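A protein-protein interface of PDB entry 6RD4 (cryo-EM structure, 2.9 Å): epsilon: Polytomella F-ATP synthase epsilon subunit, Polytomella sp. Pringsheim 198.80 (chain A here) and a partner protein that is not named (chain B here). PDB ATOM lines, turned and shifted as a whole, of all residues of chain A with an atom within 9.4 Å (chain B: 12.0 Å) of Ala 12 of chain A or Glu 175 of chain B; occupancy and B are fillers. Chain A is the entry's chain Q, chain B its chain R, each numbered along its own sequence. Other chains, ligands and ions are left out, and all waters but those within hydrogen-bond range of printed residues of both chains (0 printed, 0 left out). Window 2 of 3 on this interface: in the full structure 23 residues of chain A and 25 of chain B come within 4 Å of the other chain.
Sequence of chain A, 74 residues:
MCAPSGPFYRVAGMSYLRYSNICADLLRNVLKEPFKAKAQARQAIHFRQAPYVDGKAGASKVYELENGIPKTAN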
ATOM      1  N   ALA A   3     -10.652  -4.340  24.880  1.00  0.00           N
ATOM      2  CA  ALA A   3      -9.199  -4.250  25.000  1.00  0.00           C
ATOM      3  C   ALA A   3      -8.582  -2.900  24.560  1.00  0.00           C
ATOM      4  O   ALA A   3      -7.578  -2.495  25.146  1.00  0.00           O
ATOM      5  CB  ALA A   3      -8.536  -5.417  24.250  1.00  0.00           C
ATOM      6  N   PRO A   4      -9.126  -2.196  23.558  1.00  0.00           N
ATOM      7  CA  PRO A   4      -8.827  -0.767  23.461  1.00  0.00           C
ATOM      8  C   PRO A   4      -9.773   0.027  24.344  1.00  0.00           C
ATOM      9  O   PRO A   4     -10.839  -0.443  24.740  1.00  0.00           O
ATOM     10  CB  PRO A   4      -9.048  -0.438  21.977  1.00  0.00           C
ATOM     11  CG  PRO A   4      -9.085  -1.748  21.292  1.00  0.00           C
ATOM     12  CD  PRO A   4      -9.726  -2.650  22.287  1.00  0.00           C
ATOM     13  N   SER A   5      -9.361   1.250  24.649  1.00  0.00           N
ATOM     14  CA  SER A   5     -10.109   2.137  25.527  1.00  0.00           C
ATOM     15  C   SER A   5     -10.445   3.407  24.765  1.00  0.00           C
ATOM     16  O   SER A   5      -9.551   4.063  24.225  1.00  0.00           O
ATOM     17  CB  SER A   5      -9.306   2.456  26.788  1.00  0.00           C
ATOM     18  OG  SER A   5      -8.137   3.190  26.479  1.00  0.00           O
ATOM     19  N   GLY A   6     -11.725   3.749  24.722  1.00  0.00           N
ATOM     20  CA  GLY A   6     -12.168   4.929  24.027  1.00  0.00           C
ATOM     21  C   GLY A   6     -13.639   4.890  23.691  1.00  0.00           C
ATOM     22  O   GLY A   6     -14.454   4.340  24.435  1.00  0.00           O
ATOM     23  N   PRO A   7     -14.007   5.466  22.552  1.00  0.00           N
ATOM     24  CA  PRO A   7     -15.418   5.478  22.155  1.00  0.00           C
ATOM     25  C   PRO A   7     -15.938   4.117  21.729  1.00  0.00           C
ATOM     26  O   PRO A   7     -15.195   3.134  21.728  1.00  0.00           O
ATOM     27  CB  PRO A   7     -15.445   6.479  20.997  1.00  0.00           C
ATOM     28  CG  PRO A   7     -14.170   7.244  21.112  1.00  0.00           C
ATOM     29  CD  PRO A   7     -13.185   6.314  21.680  1.00  0.00           C
ATOM     30  N   PHE A   8     -17.220   4.053  21.369  1.00  0.00           N
ATOM     31  CA  PHE A   8     -17.861   2.764  21.156  1.00  0.00           C
ATOM     32  C   PHE A   8     -17.395   2.084  19.885  1.00  0.00           C
ATOM     33  O   PHE A   8     -17.519   0.862  19.769  1.00  0.00           O
ATOM     34  CB  PHE A   8     -19.380   2.910  21.142  1.00  0.00           C
ATOM     35  CG  PHE A   8     -19.915   3.760  20.029  1.00  0.00           C
ATOM     36  CD1 PHE A   8     -20.393   3.181  18.868  1.00  0.00           C
ATOM     37  CD2 PHE A   8     -19.998   5.134  20.168  1.00  0.00           C
ATOM     38  CE1 PHE A   8     -20.904   3.958  17.858  1.00  0.00           C
ATOM     39  CE2 PHE A   8     -20.506   5.914  19.163  1.00  0.00           C
ATOM     40  CZ  PHE A   8     -20.964   5.325  18.009  1.00  0.00           C
ATOM     41  N   TYR A   9     -16.872   2.840  18.932  1.00  0.00           N
ATOM     42  CA  TYR A   9     -16.263   2.237  17.762  1.00  0.00           C
ATOM     43  C   TYR A   9     -14.839   1.798  18.047  1.00  0.00           C
ATOM     44  O   TYR A   9     -14.401   0.761  17.549  1.00  0.00           O
ATOM     45  CB  TYR A   9     -16.296   3.214  16.583  1.00  0.00           C
ATOM     46  CG  TYR A   9     -15.845   4.618  16.899  1.00  0.00           C
ATOM     47  CD1 TYR A   9     -16.756   5.592  17.264  1.00  0.00           C
ATOM     48  CD2 TYR A   9     -14.510   4.976  16.803  1.00  0.00           C
ATOM     49  CE1 TYR A   9     -16.349   6.867  17.542  1.00  0.00           C
ATOM     50  CE2 TYR A   9     -14.099   6.247  17.085  1.00  0.00           C
ATOM     51  CZ  TYR A   9     -15.019   7.186  17.453  1.00  0.00           C
ATOM     52  OH  TYR A   9     -14.605   8.458  17.730  1.00  0.00           O
ATOM     53  N   ARG A  10     -14.120   2.551  18.874  1.00  0.00           N
ATOM     54  CA  ARG A  10     -12.709   2.269  19.087  1.00  0.00           C
ATOM     55  C   ARG A  10     -12.503   1.069  20.000  1.00  0.00           C
ATOM     56  O   ARG A  10     -11.567   0.293  19.788  1.00  0.00           O
ATOM     57  CB  ARG A  10     -12.021   3.501  19.656  1.00  0.00           C
ATOM     58  CG  ARG A  10     -10.531   3.425  19.669  1.00  0.00           C
ATOM     59  CD  ARG A  10      -9.988   3.403  18.267  1.00  0.00           C
ATOM     60  NE  ARG A  10     -10.163   4.680  17.586  1.00  0.00           N
ATOM     61  CZ  ARG A  10      -9.545   4.999  16.456  1.00  0.00           C
ATOM     62  NH1 ARG A  10      -8.709   4.139  15.899  1.00  0.00           N
ATOM     63  NH2 ARG A  10      -9.745   6.177  15.892  1.00  0.00           N
ATOM     64  N   VAL A  11     -13.371   0.884  20.998  1.00  0.00           N
ATOM     65  CA  VAL A  11     -13.273  -0.307  21.836  1.00  0.00           C
ATOM     66  C   VAL A  11     -13.765  -1.549  21.108  1.00  0.00           C
ATOM     67  O   VAL A  11     -13.413  -2.667  21.500  1.00  0.00           O
ATOM     68  CB  VAL A  11     -14.037  -0.150  23.166  1.00  0.00           C
ATOM     69  CG1 VAL A  11     -13.609   1.105  23.867  1.00  0.00           C
ATOM     70  CG2 VAL A  11     -15.540  -0.131  22.947  1.00  0.00           C
ATOM     71  N   ALA A  12     -14.544  -1.385  20.043  1.00  0.00           N
ATOM     72  CA  ALA A  12     -14.999  -2.496  19.228  1.00  0.00           C
ATOM     73  C   ALA A  12     -14.035  -2.819  18.098  1.00  0.00           C
ATOM     74  O   ALA A  12     -14.418  -3.512  17.153  1.00  0.00           O
ATOM     75  CB  ALA A  12     -16.388  -2.204  18.663  1.00  0.00           C
ATOM     76  N   GLY A  13     -12.802  -2.313  18.162  1.00  0.00           N
ATOM     77  CA  GLY A  13     -11.796  -2.563  17.152  1.00  0.00           C
ATOM     78  C   GLY A  13     -11.914  -1.715  15.907  1.00  0.00           C
ATOM     79  O   GLY A  13     -10.965  -1.673  15.116  1.00  0.00           O
ATOM     80  N   MET A  14     -13.033  -1.028  15.718  1.00  0.00           N
ATOM     81  CA  MET A  14     -13.274  -0.262  14.507  1.00  0.00           C
ATOM     82  C   MET A  14     -12.509   1.053  14.554  1.00  0.00           C
ATOM     83  O   MET A  14     -12.406   1.689  15.603  1.00  0.00           O
ATOM     84  CB  MET A  14     -14.771  -0.017  14.354  1.00  0.00           C
ATOM     85  CG  MET A  14     -15.183   0.622  13.067  1.00  0.00           C
ATOM     86  SD  MET A  14     -16.880   1.197  13.113  1.00  0.00           S
ATOM     87  CE  MET A  14     -17.720  -0.208  13.785  1.00  0.00           C
ATOM     88  N   SER A  15     -11.945   1.446  13.419  1.00  0.00           N
ATOM     89  CA  SER A  15     -11.279   2.728  13.307  1.00  0.00           C
ATOM     90  C   SER A  15     -12.314   3.839  13.179  1.00  0.00           C
ATOM     91  O   SER A  15     -13.497   3.594  12.936  1.00  0.00           O
ATOM     92  CB  SER A  15     -10.344   2.736  12.106  1.00  0.00           C
ATOM     93  OG  SER A  15     -11.081   2.843  10.902  1.00  0.00           O
ATOM     94  N   ARG A  18     -13.706   4.119   9.463  1.00  0.00           N
ATOM     95  CA  ARG A  18     -14.790   3.224   9.107  1.00  0.00           C
ATOM     96  C   ARG A  18     -16.087   3.666   9.750  1.00  0.00           C
ATOM     97  O   ARG A  18     -17.132   3.650   9.100  1.00  0.00           O
ATOM     98  CB  ARG A  18     -14.471   1.794   9.511  1.00  0.00           C
ATOM     99  CG  ARG A  18     -15.416   0.816   8.866  1.00  0.00           C
ATOM    100  CD  ARG A  18     -15.037  -0.592   9.175  1.00  0.00           C
ATOM    101  NE  ARG A  18     -13.839  -0.985   8.457  1.00  0.00           N
ATOM    102  CZ  ARG A  18     -13.859  -1.655   7.318  1.00  0.00           C
ATOM    103  NH1 ARG A  18     -15.015  -1.998   6.768  1.00  0.00           N
ATOM    104  NH2 ARG A  18     -12.722  -1.979   6.727  1.00  0.00           N
ATOM    105  N   TYR A  19     -16.022   4.107  11.005  1.00  0.00           N
ATOM    106  CA  TYR A  19     -17.213   4.546  11.718  1.00  0.00           C
ATOM    107  C   TYR A  19     -17.811   5.783  11.075  1.00  0.00           C
ATOM    108  O   TYR A  19     -19.030   5.886  10.911  1.00  0.00           O
ATOM    109  CB  TYR A  19     -16.870   4.816  13.182  1.00  0.00           C
ATOM    110  CG  TYR A  19     -17.817   5.773  13.854  1.00  0.00           C
ATOM    111  CD1 TYR A  19     -17.427   7.069  14.152  1.00  0.00           C
ATOM    112  CD2 TYR A  19     -19.099   5.381  14.190  1.00  0.00           C
ATOM    113  CE1 TYR A  19     -18.288   7.942  14.746  1.00  0.00           C
ATOM    114  CE2 TYR A  19     -19.963   6.250  14.787  1.00  0.00           C
ATOM    115  CZ  TYR A  19     -19.554   7.530  15.064  1.00  0.00           C
ATOM    116  OH  TYR A  19     -20.422   8.405  15.671  1.00  0.00           O
ATOM    117  N   LYS A  71     -20.371  -2.627   6.611  1.00  0.00           N
ATOM    118  CA  LYS A  71     -20.870  -2.463   7.969  1.00  0.00           C
ATOM    119  C   LYS A  71     -20.441  -3.589   8.890  1.00  0.00           C
ATOM    120  O   LYS A  71     -20.405  -3.394  10.109  1.00  0.00           O
ATOM    121  CB  LYS A  71     -22.396  -2.389   7.956  1.00  0.00           C
ATOM    122  CG  LYS A  71     -22.960  -1.274   7.112  1.00  0.00           C
ATOM    123  CD  LYS A  71     -24.404  -1.549   6.742  1.00  0.00           C
ATOM    124  CE  LYS A  71     -24.980  -0.409   5.928  1.00  0.00           C
ATOM    125  NZ  LYS A  71     -24.122  -0.030   4.778  1.00  0.00           N
ATOM    126  N   THR A  72     -20.107  -4.750   8.343  1.00  0.00           N
ATOM    127  CA  THR A  72     -19.755  -5.903   9.149  1.00  0.00           C
ATOM    128  C   THR A  72     -18.293  -5.830   9.576  1.00  0.00           C
ATOM    129  O   THR A  72     -17.601  -4.833   9.363  1.00  0.00           O
ATOM    130  CB  THR A  72     -20.039  -7.191   8.384  1.00  0.00           C
ATOM    131  OG1 THR A  72     -19.014  -7.398   7.402  1.00  0.00           O
ATOM    132  CG2 THR A  72     -21.384  -7.096   7.691  1.00  0.00           C
ATOM    133  N   ALA A  73     -17.820  -6.908  10.192  1.00  0.00           N
ATOM    134  CA  ALA A  73     -16.448  -6.966  10.670  1.00  0.00           C
ATOM    135  C   ALA A  73     -15.484  -7.176   9.512  1.00  0.00           C
ATOM    136  O   ALA A  73     -15.757  -7.955   8.594  1.00  0.00           O
ATOM    137  CB  ALA A  73     -16.292  -8.090  11.691  1.00  0.00           C
ATOM    138  N   ASN A  74     -14.352  -6.487   9.560  1.00  0.00           N
ATOM    139  CA  ASN A  74     -13.329  -6.606   8.529  1.00  0.00           C
ATOM    140  C   ASN A  74     -12.394  -7.780   8.806  1.00  0.00           C
ATOM    141  O   ASN A  74     -12.286  -8.710   8.005  1.00  0.00           O
ATOM    142  CB  ASN A  74     -12.532  -5.305   8.426  1.00  0.00           C
ATOM    143  CG  ASN A  74     -11.813  -4.959   9.715  1.00  0.00           C
ATOM    144  OD1 ASN A  74     -12.285  -5.270  10.809  1.00  0.00           O
ATOM    145  ND2 ASN A  74     -10.670  -4.299   9.594  1.00  0.00           N
ATOM    146  N   ALA B 170     -32.324  -5.687  14.762  1.00  0.00           N
ATOM    147  CA  ALA B 170     -31.213  -6.572  14.425  1.00  0.00           C
ATOM    148  C   ALA B 170     -29.992  -6.204  15.261  1.00  0.00           C
ATOM    149  O   ALA B 170     -29.168  -5.389  14.844  1.00  0.00           O
ATOM    150  CB  ALA B 170     -30.909  -6.493  12.933  1.00  0.00           C
ATOM    151  N   GLN B 171     -29.863  -6.824  16.431  1.00  0.00           N
ATOM    152  CA  GLN B 171     -28.668  -6.683  17.264  1.00  0.00           C
ATOM    153  C   GLN B 171     -28.160  -8.071  17.626  1.00  0.00           C
ATOM    154  O   GLN B 171     -28.605  -8.657  18.628  1.00  0.00           O
ATOM    155  CB  GLN B 171     -28.899  -5.862  18.532  1.00  0.00           C
ATOM    156  CG  GLN B 171     -29.396  -4.431  18.354  1.00  0.00           C
ATOM    157  CD  GLN B 171     -30.853  -4.341  17.990  1.00  0.00           C
ATOM    158  OE1 GLN B 171     -31.622  -5.268  18.241  1.00  0.00           O
ATOM    159  NE2 GLN B 171     -31.242  -3.231  17.386  1.00  0.00           N
ATOM    160  N   PRO B 172     -27.244  -8.625  16.845  1.00  0.00           N
ATOM    161  CA  PRO B 172     -26.646  -9.911  17.210  1.00  0.00           C
ATOM    162  C   PRO B 172     -25.443  -9.720  18.117  1.00  0.00           C
ATOM    163  O   PRO B 172     -25.136  -8.595  18.520  1.00  0.00           O
ATOM    164  CB  PRO B 172     -26.253 -10.515  15.855  1.00  0.00           C
ATOM    165  CG  PRO B 172     -26.177  -9.346  14.896  1.00  0.00           C
ATOM    166  CD  PRO B 172     -26.708  -8.113  15.575  1.00  0.00           C
ATOM    167  N   THR B 173     -24.752 -10.813  18.437  1.00  0.00           N
ATOM    168  CA  THR B 173     -23.582 -10.758  19.304  1.00  0.00           C
ATOM    169  C   THR B 173     -22.309 -10.390  18.534  1.00  0.00           C
ATOM    170  O   THR B 173     -21.202 -10.533  19.069  1.00  0.00           O
ATOM    171  CB  THR B 173     -23.431 -12.105  20.025  1.00  0.00           C
ATOM    172  OG1 THR B 173     -24.733 -12.667  20.229  1.00  0.00           O
ATOM    173  CG2 THR B 173     -22.822 -11.920  21.424  1.00  0.00           C
ATOM    174  N   ASP B 174     -22.432  -9.921  17.292  1.00  0.00           N
ATOM    175  CA  ASP B 174     -21.291  -9.367  16.572  1.00  0.00           C
ATOM    176  C   ASP B 174     -20.869  -8.056  17.229  1.00  0.00           C
ATOM    177  O   ASP B 174     -21.630  -7.084  17.237  1.00  0.00           O
ATOM    178  CB  ASP B 174     -21.648  -9.149  15.103  1.00  0.00           C
ATOM    179  CG  ASP B 174     -20.424  -8.969  14.223  1.00  0.00           C
ATOM    180  OD1 ASP B 174     -20.592  -8.804  12.998  1.00  0.00           O
ATOM    181  OD2 ASP B 174     -19.294  -9.007  14.748  1.00  0.00           O
ATOM    182  N   GLU B 175     -19.660  -8.034  17.793  1.00  0.00           N
ATOM    183  CA  GLU B 175     -19.218  -6.865  18.542  1.00  0.00           C
ATOM    184  C   GLU B 175     -18.783  -5.742  17.608  1.00  0.00           C
ATOM    185  O   GLU B 175     -18.656  -4.588  18.026  1.00  0.00           O
ATOM    186  CB  GLU B 175     -18.104  -7.255  19.515  1.00  0.00           C
ATOM    187  CG  GLU B 175     -16.808  -7.720  18.880  1.00  0.00           C
ATOM    188  CD  GLU B 175     -15.793  -6.606  18.796  1.00  0.00           C
ATOM    189  OE1 GLU B 175     -15.940  -5.643  19.573  1.00  0.00           O
ATOM    190  OE2 GLU B 175     -14.861  -6.688  17.968  1.00  0.00           O
ATOM    191  N   PHE B 176     -18.498  -6.068  16.351  1.00  0.00           N
ATOM    192  CA  PHE B 176     -18.291  -5.026  15.354  1.00  0.00           C
ATOM    193  C   PHE B 176     -19.616  -4.409  14.931  1.00  0.00           C
ATOM    194  O   PHE B 176     -19.704  -3.199  14.702  1.00  0.00           O
ATOM    195  CB  PHE B 176     -17.559  -5.605  14.155  1.00  0.00           C
ATOM    196  CG  PHE B 176     -16.732  -4.613  13.412  1.00  0.00           C
ATOM    197  CD1 PHE B 176     -15.379  -4.500  13.669  1.00  0.00           C
ATOM    198  CD2 PHE B 176     -17.297  -3.811  12.436  1.00  0.00           C
ATOM    199  CE1 PHE B 176     -14.603  -3.601  12.974  1.00  0.00           C
ATOM    200  CE2 PHE B 176     -16.530  -2.913  11.739  1.00  0.00           C
ATOM    201  CZ  PHE B 176     -15.183  -2.808  12.009  1.00  0.00           C
ATOM    202  N   GLU B 177     -20.661  -5.227  14.815  1.00  0.00           N
ATOM    203  CA  GLU B 177     -21.991  -4.690  14.583  1.00  0.00           C
ATOM    204  C   GLU B 177     -22.627  -4.176  15.866  1.00  0.00           C
ATOM    205  O   GLU B 177     -23.713  -3.600  15.807  1.00  0.00           O
ATOM    206  CB  GLU B 177     -22.889  -5.750  13.937  1.00  0.00           C
ATOM    207  CG  GLU B 177     -23.812  -5.230  12.835  1.00  0.00           C
ATOM    208  CD  GLU B 177     -25.174  -4.790  13.335  1.00  0.00           C
ATOM    209  OE1 GLU B 177     -25.614  -5.282  14.388  1.00  0.00           O
ATOM    210  OE2 GLU B 177     -25.816  -3.956  12.669  1.00  0.00           O
ATOM    211  N   GLN B 178     -21.989  -4.390  17.020  1.00  0.00           N
ATOM    212  CA  GLN B 178     -22.391  -3.698  18.238  1.00  0.00           C
ATOM    213  C   GLN B 178     -22.237  -2.194  18.071  1.00  0.00           C
ATOM    214  O   GLN B 178     -23.111  -1.415  18.467  1.00  0.00           O
ATOM    215  CB  GLN B 178     -21.560  -4.185  19.428  1.00  0.00           C
ATOM    216  CG  GLN B 178     -21.918  -3.545  20.757  1.00  0.00           C
ATOM    217  CD  GLN B 178     -23.295  -3.938  21.222  1.00  0.00           C
ATOM    218  OE1 GLN B 178     -24.259  -3.190  21.061  1.00  0.00           O
ATOM    219  NE2 GLN B 178     -23.395  -5.114  21.828  1.00  0.00           N
ATOM    220  N   ALA B 179     -21.128  -1.769  17.471  1.00  0.00           N
ATOM    221  CA  ALA B 179     -20.908  -0.346  17.251  1.00  0.00           C
ATOM    222  C   ALA B 179     -21.656   0.150  16.022  1.00  0.00           C
ATOM    223  O   ALA B 179     -22.210   1.255  16.033  1.00  0.00           O
ATOM    224  CB  ALA B 179     -19.411  -0.069  17.127  1.00  0.00           C
ATOM    225  N   ALA B 180     -21.701  -0.660  14.960  1.00  0.00           N
ATOM    226  CA  ALA B 180     -22.280  -0.209  13.696  1.00  0.00           C
ATOM    227  C   ALA B 180     -23.794  -0.114  13.777  1.00  0.00           C
ATOM    228  O   ALA B 180     -24.410   0.688  13.069  1.00  0.00           O
ATOM    229  CB  ALA B 180     -21.868  -1.141  12.561  1.00  0.00           C
ATOM    230  N   ASN B 181     -24.416  -0.934  14.617  1.00  0.00           N
ATOM    231  CA  ASN B 181     -25.840  -0.746  14.832  1.00  0.00           C
ATOM    232  C   ASN B 181     -26.085   0.408  15.790  1.00  0.00           C
ATOM    233  O   ASN B 181     -27.076   1.132  15.641  1.00  0.00           O
ATOM    234  CB  ASN B 181     -26.468  -2.029  15.358  1.00  0.00           C
ATOM    235  CG  ASN B 181     -27.946  -2.101  15.101  1.00  0.00           C
ATOM    236  OD1 ASN B 181     -28.694  -1.181  15.396  1.00  0.00           O
ATOM    237  ND2 ASN B 181     -28.378  -3.214  14.537  1.00  0.00           N
ATOM    238  N   ARG B 182     -25.187   0.606  16.762  1.00  0.00           N
ATOM    239  CA  ARG B 182     -25.283   1.762  17.649  1.00  0.00           C
ATOM    240  C   ARG B 182     -25.153   3.059  16.864  1.00  0.00           C
ATOM    241  O   ARG B 182     -25.903   4.015  17.093  1.00  0.00           O
ATOM    242  CB  ARG B 182     -24.208   1.686  18.735  1.00  0.00           C
ATOM    243  CG  ARG B 182     -24.076   2.952  19.562  1.00  0.00           C
ATOM    244  CD  ARG B 182     -23.365   2.696  20.872  1.00  0.00           C
ATOM    245  NE  ARG B 182     -23.010   3.940  21.546  1.00  0.00           N
ATOM    246  CZ  ARG B 182     -22.392   4.000  22.719  1.00  0.00           C
ATOM    247  NH1 ARG B 182     -22.055   2.886  23.346  1.00  0.00           N
ATOM    248  NH2 ARG B 182     -22.104   5.171  23.263  1.00  0.00           N
ATOM    249  N   ALA B 183     -24.234   3.085  15.898  1.00  0.00           N
ATOM    250  CA  ALA B 183     -24.114   4.233  15.011  1.00  0.00           C
ATOM    251  C   ALA B 183     -25.319   4.349  14.095  1.00  0.00           C
ATOM    252  O   ALA B 183     -25.697   5.455  13.692  1.00  0.00           O
ATOM    253  CB  ALA B 183     -22.832   4.119  14.198  1.00  0.00           C
ATOM    254  N   ALA B 184     -25.944   3.219  13.763  1.00  0.00           N
ATOM    255  CA  ALA B 184     -27.140   3.250  12.932  1.00  0.00           C
ATOM    256  C   ALA B 184     -28.324   3.823  13.693  1.00  0.00           C
ATOM    257  O   ALA B 184     -29.141   4.559  13.130  1.00  0.00           O
ATOM    258  CB  ALA B 184     -27.462   1.847  12.423  1.00  0.00           C
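The backbone carbonyl oxygen (O) of Ala 12 of chain A lies close to the side-chain carboxylate (OE2) of Glu 175 of chain B (3.3 Å).
The backbone NH of Met 14 of chain A sits at hydrogen-bond distance from the backbone carbonyl oxygen of Tyr 9 of chain A (2.9 Å).
N of Tyr 19 of chain A sits close to SD of Met 14 of chain A.
The side-chain hydroxyl (OG) of Ser 15 of chain A lies within hydrogen-bond range of the backbone NH (N) of Arg 18 of chain A (3.3 Å).
The backbone NH (N) of Phe 176 of chain B lies close to the side-chain carboxylate (OD2) of Asp 174 of chain B (3.4 Å).
Among the printed residues, pairs that only touch across the chains: Phe 8 of chain A with Ala 179 of chain B, Phe 8 of chain A with Arg 182 of chain B, Phe 8 of chain A with Ala 183 of chain B, Tyr 9 of chain A with Ala 179 of chain B, Ala 12 of chain A with Phe 176 of chain B, Met 14 of chain A with Phe 176 of chain B, Met 14 of chain A with Ala 179 of chain B, Arg 18 of chain A with Phe 176 of chain B, Tyr 19 of chain A with Ala 183 of chain B, Lys 71 of chain A with Phe 176 of chain B, Lys 71 of chain A with Ala 180 of chain B, Thr 72 of chain A with Phe 176 of chain B, Ala 73 of chain A with Phe 176 of chain B and Asn 74 of chain A with Phe 176 of chain B.
No residue of chain B comes within 4 Å of Pro 4 of chain A.
Ser 5 of chain A touches none of the printed residues of chain B.
Arg 10 of chain A touches none of the printed residues of chain B.
No residue of chain B comes within 4 Å of Val 11 of chain A.
Of the printed residues of chain B, Ala 12 of chain A touches Glu 175 and Phe 176.
No residue of chain B comes within 4 Å of Gly 13 of chain A.
Of chain B, only Phe 176 (3.6 Å) and Ala 179 (3.7 Å) come within 4 Å of Met 14 of chain A.
Of the printed residues of chain B, Lys 71 of chain A touches Phe 176 (3.9 Å) and Ala 180 (3.6 Å).
Of the printed residues of chain B, Ala 73 of chain A touches Phe 176 (3.6 Å).
No residue of chain A comes within 4 Å of Asp 174 of chain B.
Of chain A, only Ala 12 comes within 4 Å of Glu 175 of chain B.
Printed residues of chain A within 4 Å of Phe 176 of chain B: Ala 12, Met 14, Arg 18, Lys 71, Thr 72, Ala 73 and Asn 74.
The nearest printed residue of chain B that does not touch Ala 12 of chain A is Ala 179 of chain B (4.01 Å).
The nearest residue of chain A that does not touch Glu 175 of chain B is Val 11 of chain A (4.4 Å).
Hydrophobic or aromatic side chains of chain B that line the printed part of chain A: Phe 176, Ala 179, Ala 180 and Ala 183.
Along chain B the printed residues that touch a printed residue of chain A span positions 175 to 183.
Of the 19 printed residues of chain A, 10 touch a printed residue of chain B.
Among the printed residues, no Asp or Glu carboxylate lies within 4 Å of a Lys or Arg side-chain nitrogen of the other chain.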
